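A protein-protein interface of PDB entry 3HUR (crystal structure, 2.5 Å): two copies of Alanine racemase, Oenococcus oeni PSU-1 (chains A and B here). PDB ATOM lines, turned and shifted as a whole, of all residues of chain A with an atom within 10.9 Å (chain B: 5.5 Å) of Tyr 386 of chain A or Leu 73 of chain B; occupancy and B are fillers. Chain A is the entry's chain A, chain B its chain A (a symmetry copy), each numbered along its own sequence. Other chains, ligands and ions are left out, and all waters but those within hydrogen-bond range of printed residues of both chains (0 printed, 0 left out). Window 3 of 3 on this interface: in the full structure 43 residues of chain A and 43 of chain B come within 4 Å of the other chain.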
ATOM      1  N   ARG A   8      12.433 -34.022  20.335  1.00  0.00           N
ATOM      2  CA  ARG A   8      12.913 -33.781  21.723  1.00  0.00           C
ATOM      3  C   ARG A   8      11.709 -33.756  22.709  1.00  0.00           C
ATOM      4  O   ARG A   8      11.270 -32.680  23.137  1.00  0.00           O
ATOM      5  CB  ARG A   8      13.650 -32.424  21.748  1.00  0.00           C
ATOM      6  CG  ARG A   8      14.109 -31.915  23.109  1.00  0.00           C
ATOM      7  CD  ARG A   8      15.569 -32.125  23.335  1.00  0.00           C
ATOM      8  NE  ARG A   8      16.441 -31.510  22.325  1.00  0.00           N
ATOM      9  CZ  ARG A   8      17.545 -32.090  21.847  1.00  0.00           C
ATOM     10  NH1 ARG A   8      18.285 -31.470  20.928  1.00  0.00           N
ATOM     11  NH2 ARG A   8      17.916 -33.307  22.267  1.00  0.00           N
ATOM     12  N   TRP A  11      13.051 -33.364  28.267  1.00  0.00           N
ATOM     13  CA  TRP A  11      14.334 -32.749  28.521  1.00  0.00           C
ATOM     14  C   TRP A  11      14.441 -32.237  29.978  1.00  0.00           C
ATOM     15  O   TRP A  11      13.433 -32.140  30.685  1.00  0.00           O
ATOM     16  CB  TRP A  11      14.551 -31.604  27.534  1.00  0.00           C
ATOM     17  CG  TRP A  11      13.591 -30.487  27.656  1.00  0.00           C
ATOM     18  CD1 TRP A  11      13.730 -29.368  28.411  1.00  0.00           C
ATOM     19  CD2 TRP A  11      12.327 -30.360  26.976  1.00  0.00           C
ATOM     20  NE1 TRP A  11      12.609 -28.554  28.272  1.00  0.00           N
ATOM     21  CE2 TRP A  11      11.739 -29.151  27.401  1.00  0.00           C
ATOM     22  CE3 TRP A  11      11.634 -31.159  26.053  1.00  0.00           C
ATOM     23  CZ2 TRP A  11      10.530 -28.716  26.923  1.00  0.00           C
ATOM     24  CZ3 TRP A  11      10.421 -30.737  25.612  1.00  0.00           C
ATOM     25  CH2 TRP A  11       9.878 -29.522  26.031  1.00  0.00           C
ATOM     26  N   VAL A  14      17.247 -26.285  32.840  1.00  0.00           N
ATOM     27  CA  VAL A  14      18.165 -25.777  33.827  1.00  0.00           C
ATOM     28  C   VAL A  14      18.189 -24.229  33.776  1.00  0.00           C
ATOM     29  O   VAL A  14      18.630 -23.629  32.797  1.00  0.00           O
ATOM     30  CB  VAL A  14      19.598 -26.264  33.531  1.00  0.00           C
ATOM     31  CG1 VAL A  14      20.560 -25.668  34.553  1.00  0.00           C
ATOM     32  CG2 VAL A  14      19.682 -27.800  33.481  1.00  0.00           C
ATOM     33  N   LEU A  16      19.728 -20.935  34.617  1.00  0.00           N
ATOM     34  CA  LEU A  16      21.058 -20.522  35.052  1.00  0.00           C
ATOM     35  C   LEU A  16      21.012 -19.320  35.924  1.00  0.00           C
ATOM     36  O   LEU A  16      21.935 -19.124  36.706  1.00  0.00           O
ATOM     37  CB  LEU A  16      21.988 -20.249  33.871  1.00  0.00           C
ATOM     38  CG  LEU A  16      22.369 -21.479  33.032  1.00  0.00           C
ATOM     39  CD1 LEU A  16      23.124 -21.104  31.755  1.00  0.00           C
ATOM     40  CD2 LEU A  16      23.166 -22.465  33.886  1.00  0.00           C
ATOM     41  N   ILE A  49      30.102 -26.311  31.951  1.00  0.00           N
ATOM     42  CA  ILE A  49      30.434 -25.163  31.137  1.00  0.00           C
ATOM     43  C   ILE A  49      29.406 -24.044  31.237  1.00  0.00           C
ATOM     44  O   ILE A  49      29.772 -22.961  31.643  1.00  0.00           O
ATOM     45  CB  ILE A  49      30.629 -25.608  29.713  1.00  0.00           C
ATOM     46  CG1 ILE A  49      31.728 -26.642  29.698  1.00  0.00           C
ATOM     47  CG2 ILE A  49      30.957 -24.463  28.803  1.00  0.00           C
ATOM     48  CD1 ILE A  49      32.722 -26.453  28.668  1.00  0.00           C
ATOM     49  N   PRO A  50      28.123 -24.298  30.890  1.00  0.00           N
ATOM     50  CA  PRO A  50      27.088 -23.289  31.032  1.00  0.00           C
ATOM     51  C   PRO A  50      26.972 -22.738  32.450  1.00  0.00           C
ATOM     52  O   PRO A  50      26.788 -21.547  32.620  1.00  0.00           O
ATOM     53  CB  PRO A  50      25.800 -24.018  30.629  1.00  0.00           C
ATOM     54  CG  PRO A  50      26.189 -25.353  30.219  1.00  0.00           C
ATOM     55  CD  PRO A  50      27.646 -25.447  30.121  1.00  0.00           C
ATOM     56  N   LYS A  53      30.151 -20.472  32.879  1.00  0.00           N
ATOM     57  CA  LYS A  53      29.957 -19.231  32.160  1.00  0.00           C
ATOM     58  C   LYS A  53      28.952 -18.336  32.872  1.00  0.00           C
ATOM     59  O   LYS A  53      29.156 -17.142  32.958  1.00  0.00           O
ATOM     60  CB  LYS A  53      29.428 -19.469  30.754  1.00  0.00           C
ATOM     61  CG  LYS A  53      30.429 -19.993  29.784  1.00  0.00           C
ATOM     62  CD  LYS A  53      29.731 -20.247  28.458  1.00  0.00           C
ATOM     63  CE  LYS A  53      30.699 -20.675  27.364  1.00  0.00           C
ATOM     64  NZ  LYS A  53      31.480 -19.510  26.808  1.00  0.00           N
ATOM     65  N   ALA A  78      36.573 -23.270  26.545  1.00  0.00           N
ATOM     66  CA  ALA A  78      35.268 -22.584  26.425  1.00  0.00           C
ATOM     67  C   ALA A  78      35.326 -21.131  26.835  1.00  0.00           C
ATOM     68  O   ALA A  78      34.276 -20.494  26.981  1.00  0.00           O
ATOM     69  CB  ALA A  78      34.224 -23.304  27.201  1.00  0.00           C
ATOM     70  N   LYS A 371      18.497 -34.487  27.100  1.00  0.00           N
ATOM     71  CA  LYS A 371      19.340 -33.355  26.899  1.00  0.00           C
ATOM     72  C   LYS A 371      19.061 -32.309  27.957  1.00  0.00           C
ATOM     73  O   LYS A 371      17.937 -32.181  28.441  1.00  0.00           O
ATOM     74  CB  LYS A 371      19.074 -32.760  25.516  1.00  0.00           C
ATOM     75  CG  LYS A 371      19.902 -31.516  25.191  1.00  0.00           C
ATOM     76  CD  LYS A 371      20.724 -31.705  23.940  1.00  0.00           C
ATOM     77  CE  LYS A 371      21.492 -30.433  23.541  1.00  0.00           C
ATOM     78  NZ  LYS A 371      22.570 -30.829  22.576  1.00  0.00           N
ATOM     79  N   ARG A 372      20.084 -31.541  28.272  1.00  0.00           N
ATOM     80  CA  ARG A 372      19.942 -30.415  29.135  1.00  0.00           C
ATOM     81  C   ARG A 372      19.653 -29.186  28.274  1.00  0.00           C
ATOM     82  O   ARG A 372      20.412 -28.905  27.368  1.00  0.00           O
ATOM     83  CB  ARG A 372      21.222 -30.231  29.955  1.00  0.00           C
ATOM     84  CG  ARG A 372      21.267 -31.044  31.218  1.00  0.00           C
ATOM     85  CD  ARG A 372      21.090 -32.515  31.016  1.00  0.00           C
ATOM     86  NE  ARG A 372      21.301 -33.198  32.287  1.00  0.00           N
ATOM     87  CZ  ARG A 372      20.789 -34.377  32.663  1.00  0.00           C
ATOM     88  NH1 ARG A 372      20.037 -35.110  31.875  1.00  0.00           N
ATOM     89  NH2 ARG A 372      21.069 -34.835  33.868  1.00  0.00           N
ATOM     90  N   ILE A 373      18.548 -28.487  28.573  1.00  0.00           N
ATOM     91  CA  ILE A 373      18.169 -27.245  27.940  1.00  0.00           C
ATOM     92  C   ILE A 373      18.316 -26.067  28.941  1.00  0.00           C
ATOM     93  O   ILE A 373      17.884 -26.156  30.086  1.00  0.00           O
ATOM     94  CB  ILE A 373      16.702 -27.340  27.450  1.00  0.00           C
ATOM     95  CG1 ILE A 373      16.552 -28.494  26.408  1.00  0.00           C
ATOM     96  CG2 ILE A 373      16.197 -26.012  26.849  1.00  0.00           C
ATOM     97  CD1 ILE A 373      17.584 -28.531  25.277  1.00  0.00           C
ATOM     98  N   TYR A 374      18.909 -24.962  28.509  1.00  0.00           N
ATOM     99  CA  TYR A 374      19.126 -23.847  29.417  1.00  0.00           C
ATOM    100  C   TYR A 374      18.133 -22.731  29.161  1.00  0.00           C
ATOM    101  O   TYR A 374      18.011 -22.256  28.037  1.00  0.00           O
ATOM    102  CB  TYR A 374      20.584 -23.387  29.318  1.00  0.00           C
ATOM    103  CG  TYR A 374      21.495 -24.535  29.610  1.00  0.00           C
ATOM    104  CD1 TYR A 374      21.978 -25.358  28.594  1.00  0.00           C
ATOM    105  CD2 TYR A 374      21.804 -24.867  30.923  1.00  0.00           C
ATOM    106  CE1 TYR A 374      22.776 -26.479  28.886  1.00  0.00           C
ATOM    107  CE2 TYR A 374      22.610 -25.953  31.227  1.00  0.00           C
ATOM    108  CZ  TYR A 374      23.079 -26.756  30.236  1.00  0.00           C
ATOM    109  OH  TYR A 374      23.843 -27.814  30.618  1.00  0.00           O
ATOM    110  N   THR A 375      17.440 -22.301  30.210  1.00  0.00           N
ATOM    111  CA  THR A 375      16.468 -21.185  30.110  1.00  0.00           C
ATOM    112  C   THR A 375      16.930 -19.980  30.887  1.00  0.00           C
ATOM    113  O   THR A 375      17.845 -20.089  31.685  1.00  0.00           O
ATOM    114  CB  THR A 375      15.129 -21.536  30.745  1.00  0.00           C
ATOM    115  OG1 THR A 375      15.327 -21.712  32.151  1.00  0.00           O
ATOM    116  CG2 THR A 375      14.538 -22.820  30.138  1.00  0.00           C
ATOM    117  N   GLY A 376      16.269 -18.843  30.647  1.00  0.00           N
ATOM    118  CA  GLY A 376      16.474 -17.594  31.401  1.00  0.00           C
ATOM    119  C   GLY A 376      17.389 -16.594  30.722  1.00  0.00           C
ATOM    120  O   GLY A 376      18.123 -16.944  29.815  1.00  0.00           O
ATOM    121  N   ASP A 377      17.337 -15.340  31.180  1.00  0.00           N
ATOM    122  CA  ASP A 377      18.049 -14.216  30.549  1.00  0.00           C
ATOM    123  C   ASP A 377      19.534 -14.482  30.565  1.00  0.00           C
ATOM    124  O   ASP A 377      20.230 -14.270  29.580  1.00  0.00           O
ATOM    125  CB  ASP A 377      17.765 -12.882  31.290  1.00  0.00           C
ATOM    126  CG  ASP A 377      16.291 -12.385  31.147  1.00  0.00           C
ATOM    127  OD1 ASP A 377      15.557 -12.793  30.202  1.00  0.00           O
ATOM    128  OD2 ASP A 377      15.871 -11.544  31.986  1.00  0.00           O
ATOM    129  N   LEU A 378      20.040 -14.955  31.689  1.00  0.00           N
ATOM    130  CA  LEU A 378      21.467 -15.313  31.749  1.00  0.00           C
ATOM    131  C   LEU A 378      21.866 -16.308  30.660  1.00  0.00           C
ATOM    132  O   LEU A 378      22.928 -16.210  30.077  1.00  0.00           O
ATOM    133  CB  LEU A 378      21.794 -15.923  33.104  1.00  0.00           C
ATOM    134  CG  LEU A 378      22.924 -15.348  33.942  1.00  0.00           C
ATOM    135  CD1 LEU A 378      23.187 -16.345  35.071  1.00  0.00           C
ATOM    136  CD2 LEU A 378      24.166 -15.074  33.097  1.00  0.00           C
ATOM    137  N   ALA A 379      21.002 -17.277  30.400  1.00  0.00           N
ATOM    138  CA  ALA A 379      21.216 -18.258  29.361  1.00  0.00           C
ATOM    139  C   ALA A 379      21.383 -17.659  27.954  1.00  0.00           C
ATOM    140  O   ALA A 379      22.243 -18.096  27.190  1.00  0.00           O
ATOM    141  CB  ALA A 379      20.077 -19.242  29.360  1.00  0.00           C
ATOM    142  N   GLU A 380      20.536 -16.690  27.633  1.00  0.00           N
ATOM    143  CA  GLU A 380      20.583 -15.892  26.392  1.00  0.00           C
ATOM    144  C   GLU A 380      21.954 -15.213  26.292  1.00  0.00           C
ATOM    145  O   GLU A 380      22.689 -15.418  25.297  1.00  0.00           O
ATOM    146  CB  GLU A 380      19.453 -14.836  26.470  1.00  0.00           C
ATOM    147  CG  GLU A 380      18.783 -14.284  25.198  1.00  0.00           C
ATOM    148  CD  GLU A 380      17.666 -13.186  25.535  1.00  0.00           C
ATOM    149  OE1 GLU A 380      17.647 -12.576  26.658  1.00  0.00           O
ATOM    150  OE2 GLU A 380      16.796 -12.926  24.659  1.00  0.00           O
ATOM    151  N   VAL A 381      22.316 -14.470  27.355  1.00  0.00           N
ATOM    152  CA  VAL A 381      23.556 -13.683  27.399  1.00  0.00           C
ATOM    153  C   VAL A 381      24.821 -14.522  27.218  1.00  0.00           C
ATOM    154  O   VAL A 381      25.767 -14.072  26.557  1.00  0.00           O
ATOM    155  CB  VAL A 381      23.710 -12.889  28.751  1.00  0.00           C
ATOM    156  CG1 VAL A 381      25.147 -12.329  28.907  1.00  0.00           C
ATOM    157  CG2 VAL A 381      22.637 -11.769  28.905  1.00  0.00           C
ATOM    158  N   ILE A 382      24.874 -15.735  27.788  1.00  0.00           N
ATOM    159  CA  ILE A 382      26.096 -16.557  27.635  1.00  0.00           C
ATOM    160  C   ILE A 382      26.096 -17.446  26.380  1.00  0.00           C
ATOM    161  O   ILE A 382      27.066 -18.161  26.115  1.00  0.00           O
ATOM    162  CB  ILE A 382      26.415 -17.362  28.913  1.00  0.00           C
ATOM    163  CG1 ILE A 382      25.342 -18.419  29.182  1.00  0.00           C
ATOM    164  CG2 ILE A 382      26.504 -16.433  30.093  1.00  0.00           C
ATOM    165  CD1 ILE A 382      25.824 -19.543  30.028  1.00  0.00           C
ATOM    166  N   GLY A 383      25.021 -17.381  25.602  1.00  0.00           N
ATOM    167  CA  GLY A 383      24.956 -18.065  24.305  1.00  0.00           C
ATOM    168  C   GLY A 383      24.567 -19.532  24.385  1.00  0.00           C
ATOM    169  O   GLY A 383      24.980 -20.328  23.549  1.00  0.00           O
ATOM    170  N   ALA A 384      23.779 -19.894  25.395  1.00  0.00           N
ATOM    171  CA  ALA A 384      23.409 -21.283  25.636  1.00  0.00           C
ATOM    172  C   ALA A 384      21.916 -21.511  25.415  1.00  0.00           C
ATOM    173  O   ALA A 384      21.472 -22.640  25.516  1.00  0.00           O
ATOM    174  CB  ALA A 384      23.788 -21.677  27.043  1.00  0.00           C
ATOM    175  N   ASN A 385      21.155 -20.445  25.130  1.00  0.00           N
ATOM    176  CA  ASN A 385      19.682 -20.501  24.946  1.00  0.00           C
ATOM    177  C   ASN A 385      19.338 -20.305  23.499  1.00  0.00           C
ATOM    178  O   ASN A 385      19.156 -19.166  23.062  1.00  0.00           O
ATOM    179  CB  ASN A 385      18.952 -19.406  25.735  1.00  0.00           C
ATOM    180  N   TYR A 386      19.256 -21.422  22.777  1.00  0.00           N
ATOM    181  CA  TYR A 386      18.859 -21.489  21.354  1.00  0.00           C
ATOM    182  C   TYR A 386      17.344 -21.762  21.305  1.00  0.00           C
ATOM    183  O   TYR A 386      16.671 -21.536  20.293  1.00  0.00           O
ATOM    184  CB  TYR A 386      19.637 -22.620  20.623  1.00  0.00           C
ATOM    185  CG  TYR A 386      21.069 -22.875  21.151  1.00  0.00           C
ATOM    186  CD1 TYR A 386      21.301 -23.762  22.229  1.00  0.00           C
ATOM    187  CD2 TYR A 386      22.176 -22.231  20.587  1.00  0.00           C
ATOM    188  CE1 TYR A 386      22.593 -23.987  22.740  1.00  0.00           C
ATOM    189  CE2 TYR A 386      23.480 -22.460  21.083  1.00  0.00           C
ATOM    190  CZ  TYR A 386      23.683 -23.333  22.165  1.00  0.00           C
ATOM    191  OH  TYR A 386      24.967 -23.557  22.652  1.00  0.00           O
ATOM    192  N   LEU B  69      16.912 -28.192  15.528  1.00  0.00           N
ATOM    193  CA  LEU B  69      17.491 -26.907  15.280  1.00  0.00           C
ATOM    194  C   LEU B  69      18.592 -26.582  16.311  1.00  0.00           C
ATOM    195  O   LEU B  69      19.717 -26.227  15.959  1.00  0.00           O
ATOM    196  CB  LEU B  69      16.378 -25.876  15.368  1.00  0.00           C
ATOM    197  CG  LEU B  69      16.784 -24.456  15.021  1.00  0.00           C
ATOM    198  CD1 LEU B  69      17.388 -24.433  13.631  1.00  0.00           C
ATOM    199  CD2 LEU B  69      15.558 -23.520  15.171  1.00  0.00           C
ATOM    200  N   ASP B  70      18.278 -26.728  17.586  1.00  0.00           N
ATOM    201  CA  ASP B  70      19.220 -26.329  18.621  1.00  0.00           C
ATOM    202  C   ASP B  70      20.566 -27.066  18.485  1.00  0.00           C
ATOM    203  O   ASP B  70      21.599 -26.434  18.623  1.00  0.00           O
ATOM    204  CB  ASP B  70      18.570 -26.287  20.024  1.00  0.00           C
ATOM    205  CG  ASP B  70      18.611 -27.618  20.786  1.00  0.00           C
ATOM    206  OD1 ASP B  70      18.565 -28.718  20.177  1.00  0.00           O
ATOM    207  OD2 ASP B  70      18.679 -27.543  22.050  1.00  0.00           O
ATOM    208  N   GLU B  71      20.595 -28.321  18.054  1.00  0.00           N
ATOM    209  CA  GLU B  71      21.881 -28.955  17.688  1.00  0.00           C
ATOM    210  C   GLU B  71      22.610 -28.297  16.505  1.00  0.00           C
ATOM    211  O   GLU B  71      23.848 -28.289  16.449  1.00  0.00           O
ATOM    212  CB  GLU B  71      21.709 -30.444  17.397  1.00  0.00           C
ATOM    213  CG  GLU B  71      23.007 -31.252  17.393  1.00  0.00           C
ATOM    214  CD  GLU B  71      23.714 -31.277  18.776  1.00  0.00           C
ATOM    215  OE1 GLU B  71      23.084 -30.916  19.816  1.00  0.00           O
ATOM    216  OE2 GLU B  71      24.924 -31.625  18.819  1.00  0.00           O
ATOM    217  N   ALA B  72      21.850 -27.788  15.528  1.00  0.00           N
ATOM    218  CA  ALA B  72      22.462 -27.054  14.374  1.00  0.00           C
ATOM    219  C   ALA B  72      23.165 -25.818  14.903  1.00  0.00           C
ATOM    220  O   ALA B  72      24.323 -25.645  14.679  1.00  0.00           O
ATOM    221  CB  ALA B  72      21.432 -26.688  13.359  1.00  0.00           C
ATOM    222  N   LEU B  73      22.444 -25.033  15.690  1.00  0.00           N
ATOM    223  CA  LEU B  73      22.969 -23.810  16.309  1.00  0.00           C
ATOM    224  C   LEU B  73      24.224 -24.054  17.153  1.00  0.00           C
ATOM    225  O   LEU B  73      25.187 -23.331  17.009  1.00  0.00           O
ATOM    226  CB  LEU B  73      21.863 -23.098  17.111  1.00  0.00           C
ATOM    227  CG  LEU B  73      20.652 -22.667  16.235  1.00  0.00           C
ATOM    228  CD1 LEU B  73      19.671 -21.741  16.935  1.00  0.00           C
ATOM    229  CD2 LEU B  73      21.077 -22.015  14.963  1.00  0.00           C
ATOM    230  N   GLU B  74      24.241 -25.116  17.954  1.00  0.00           N
ATOM    231  CA  GLU B  74      25.414 -25.475  18.719  1.00  0.00           C
ATOM    232  C   GLU B  74      26.584 -25.854  17.868  1.00  0.00           C
ATOM    233  O   GLU B  74      27.712 -25.552  18.181  1.00  0.00           O
ATOM    234  CB  GLU B  74      25.135 -26.704  19.608  1.00  0.00           C
ATOM    235  CG  GLU B  74      24.331 -26.513  20.905  1.00  0.00           C
ATOM    236  CD  GLU B  74      24.070 -27.881  21.613  1.00  0.00           C
ATOM    237  OE1 GLU B  74      24.964 -28.445  22.338  1.00  0.00           O
ATOM    238  OE2 GLU B  74      22.972 -28.402  21.387  1.00  0.00           O
ATOM    239  N   LEU B  75      26.347 -26.658  16.858  1.00  0.00           N
ATOM    240  CA  LEU B  75      27.393 -26.997  15.921  1.00  0.00           C
ATOM    241  C   LEU B  75      27.978 -25.688  15.320  1.00  0.00           C
ATOM    242  O   LEU B  75      29.194 -25.544  15.176  1.00  0.00           O
ATOM    243  CB  LEU B  75      26.832 -27.938  14.843  1.00  0.00           C
ATOM    244  CG  LEU B  75      26.585 -29.432  15.191  1.00  0.00           C
ATOM    245  CD1 LEU B  75      25.721 -30.140  14.123  1.00  0.00           C
ATOM    246  CD2 LEU B  75      27.931 -30.165  15.295  1.00  0.00           C
ATOM    247  N   ARG B  76      27.118 -24.717  15.018  1.00  0.00           N
ATOM    248  CA  ARG B  76      27.589 -23.457  14.408  1.00  0.00           C
ATOM    249  C   ARG B  76      28.483 -22.708  15.369  1.00  0.00           C
ATOM    250  O   ARG B  76      29.568 -22.294  15.003  1.00  0.00           O
ATOM    251  CB  ARG B  76      26.425 -22.557  13.961  1.00  0.00           C
ATOM    252  CG  ARG B  76      25.714 -23.050  12.741  1.00  0.00           C
ATOM    253  CD  ARG B  76      26.622 -22.960  11.514  1.00  0.00           C
ATOM    254  NE  ARG B  76      25.943 -23.429  10.296  1.00  0.00           N
ATOM    255  CZ  ARG B  76      26.512 -24.206   9.399  1.00  0.00           C
ATOM    256  NH1 ARG B  76      27.748 -24.617   9.565  1.00  0.00           N
ATOM    257  NH2 ARG B  76      25.846 -24.618   8.347  1.00  0.00           N
ATOM    258  N   GLN B  77      28.012 -22.572  16.611  1.00  0.00           N
ATOM    259  CA  GLN B  77      28.821 -22.070  17.697  1.00  0.00           C
ATOM    260  C   GLN B  77      30.167 -22.756  17.823  1.00  0.00           C
ATOM    261  O   GLN B  77      31.122 -22.117  18.249  1.00  0.00           O
ATOM    262  CB  GLN B  77      28.128 -22.267  19.034  1.00  0.00           C
ATOM    263  CG  GLN B  77      27.103 -21.227  19.405  1.00  0.00           C
ATOM    264  CD  GLN B  77      26.873 -21.187  20.924  1.00  0.00           C
ATOM    265  OE1 GLN B  77      27.104 -22.191  21.640  1.00  0.00           O
ATOM    266  NE2 GLN B  77      26.421 -20.037  21.417  1.00  0.00           N
ATOM    267  N   ALA B  78      30.249 -24.053  17.523  1.00  0.00           N
ATOM    268  CA  ALA B  78      31.527 -24.782  17.666  1.00  0.00           C
ATOM    269  C   ALA B  78      32.419 -24.652  16.452  1.00  0.00           C
ATOM    270  O   ALA B  78      33.419 -25.370  16.348  1.00  0.00           O
ATOM    271  CB  ALA B  78      31.281 -26.215  17.981  1.00  0.00           C
ATOM    272  N   LEU B  97      16.487 -17.824  11.031  1.00  0.00           N
ATOM    273  CA  LEU B  97      17.566 -18.600  11.634  1.00  0.00           C
ATOM    274  C   LEU B  97      18.166 -19.520  10.605  1.00  0.00           C
ATOM    275  O   LEU B  97      19.380 -19.558  10.434  1.00  0.00           O
ATOM    276  CB  LEU B  97      17.076 -19.411  12.839  1.00  0.00           C
ATOM    277  CG  LEU B  97      16.993 -18.617  14.134  1.00  0.00           C
ATOM    278  CD1 LEU B  97      16.440 -19.511  15.235  1.00  0.00           C
ATOM    279  CD2 LEU B  97      18.365 -18.004  14.512  1.00  0.00           C
ATOM    280  N   HIS B 101      22.187 -18.989   9.278  1.00  0.00           N
ATOM    281  CA  HIS B 101      23.131 -20.005   9.745  1.00  0.00           C
ATOM    282  C   HIS B 101      23.373 -21.136   8.735  1.00  0.00           C
ATOM    283  O   HIS B 101      23.994 -22.161   9.088  1.00  0.00           O
ATOM    284  CB  HIS B 101      22.629 -20.589  11.076  1.00  0.00           C
ATOM    285  CG  HIS B 101      22.557 -19.586  12.182  1.00  0.00           C
ATOM    286  ND1 HIS B 101      23.683 -19.098  12.816  1.00  0.00           N
ATOM    287  CD2 HIS B 101      21.493 -19.011  12.793  1.00  0.00           C
ATOM    288  CE1 HIS B 101      23.309 -18.251  13.761  1.00  0.00           C
ATOM    289  NE2 HIS B 101      21.986 -18.181  13.766  1.00  0.00           N
ATOM    290  N   ILE B 103      21.352 -23.370   7.146  1.00  0.00           N
ATOM    291  CA  ILE B 103      20.763 -24.622   7.525  1.00  0.00           C
ATOM    292  C   ILE B 103      19.759 -25.047   6.485  1.00  0.00           C
ATOM    293  O   ILE B 103      18.847 -24.281   6.149  1.00  0.00           O
ATOM    294  CB  ILE B 103      20.024 -24.508   8.888  1.00  0.00           C
ATOM    295  CG1 ILE B 103      21.025 -24.154   9.997  1.00  0.00           C
ATOM    296  CG2 ILE B 103      19.253 -25.794   9.196  1.00  0.00           C
ATOM    297  CD1 ILE B 103      20.394 -24.062  11.361  1.00  0.00           C
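The guanidinium group (NH1) of Arg 8 of chain A lies within salt-bridge range of the side-chain carboxylate (OD1) of Asp 70 of chain B, 2.9 Å away.
The side-chain amino group of Lys 371 of chain A is in salt-bridge range of the side-chain carboxylate of Glu 71 of chain B, at 2.8 Å.
OE2 of Glu 74 of chain B is in salt-bridge range of NZ of Lys 371 of chain A.
O of Gly 383 of chain A sits at hydrogen-bond distance from NE2 of Gln 77 of chain B (2.6 Å).
The side-chain hydroxyl of Tyr 386 of chain A sits at hydrogen-bond distance from the side-chain amide oxygen of Gln 77 of chain B (2.7 Å).
N of Val 14 of chain A lies within hydrogen-bond range of O of Ile 373 of chain A (2.8 Å).
The backbone carbonyl oxygen (O) of Gly 383 of chain A sits at hydrogen-bond distance from the side-chain hydroxyl (OH) of Tyr 386 of chain A, at 3.4 Å.
Among the printed residues, merely in contact across the chains: Tyr 386 of chain A with Glu 74 of chain B (3.5 Å), Ile 373 of chain A with Asp 70 of chain B (3.5 Å), Tyr 386 of chain A with Leu 73 of chain B (3.6 Å) and Tyr 386 of chain A with Asp 70 of chain B (3.9 Å).
Printed residues of chain B within 4 Å of Arg 8 of chain A: Asp 70.
Printed residues of chain B within 4 Å of Ile 373 of chain A: Asp 70.
Printed residues of chain B within 4 Å of Gly 383 of chain A: Gln 77 (2.6 Å).
Tyr 386 of chain A touches four residues of chain B.
No residue of chain A comes within 4 Å of Leu 69 of chain B.
Printed residues of chain A within 4 Å of Glu 71 of chain B: Lys 371 (2.8 Å).
No residue of chain A comes within 4 Å of Ala 72 of chain B.
Printed residues of chain A within 4 Å of Leu 73 of chain B: Tyr 386 (3.6 Å).
Glu 74 of chain B touches just these residues of chain A: Lys 371 (2.7 Å) and Tyr 386 (3.5 Å).
Gln 77 of chain B touches two residues of chain A.
No residue of chain A comes within 4 Å of His 101 of chain B.
The nearest residue of chain A that does not touch Leu 73 of chain B is Asn 385 of chain A (6.7 Å).
Hydrophobic or aromatic side chains of chain A within 4 Å of the printed part of chain B: Ile 373 and Tyr 386.
Hydrophobic or aromatic side chains of chain B within 4 Å of the printed part of chain A: Leu 73.
Among the printed residues, Asp or Glu carboxylates within 4 Å of a Lys or Arg side-chain nitrogen of the other chain: Arg 8 of chain A with Asp 70 of chain B (2.9 Å), Lys 371 of chain A with Glu 71 of chain B (2.8 Å) and Lys 371 of chain A with Glu 74 of chain B (2.7 Å).
Position printed for both chains: 78.
Of the 9 pairs that touch across the chains among the printed residues, none has its exchanged pair printed and touching as well.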
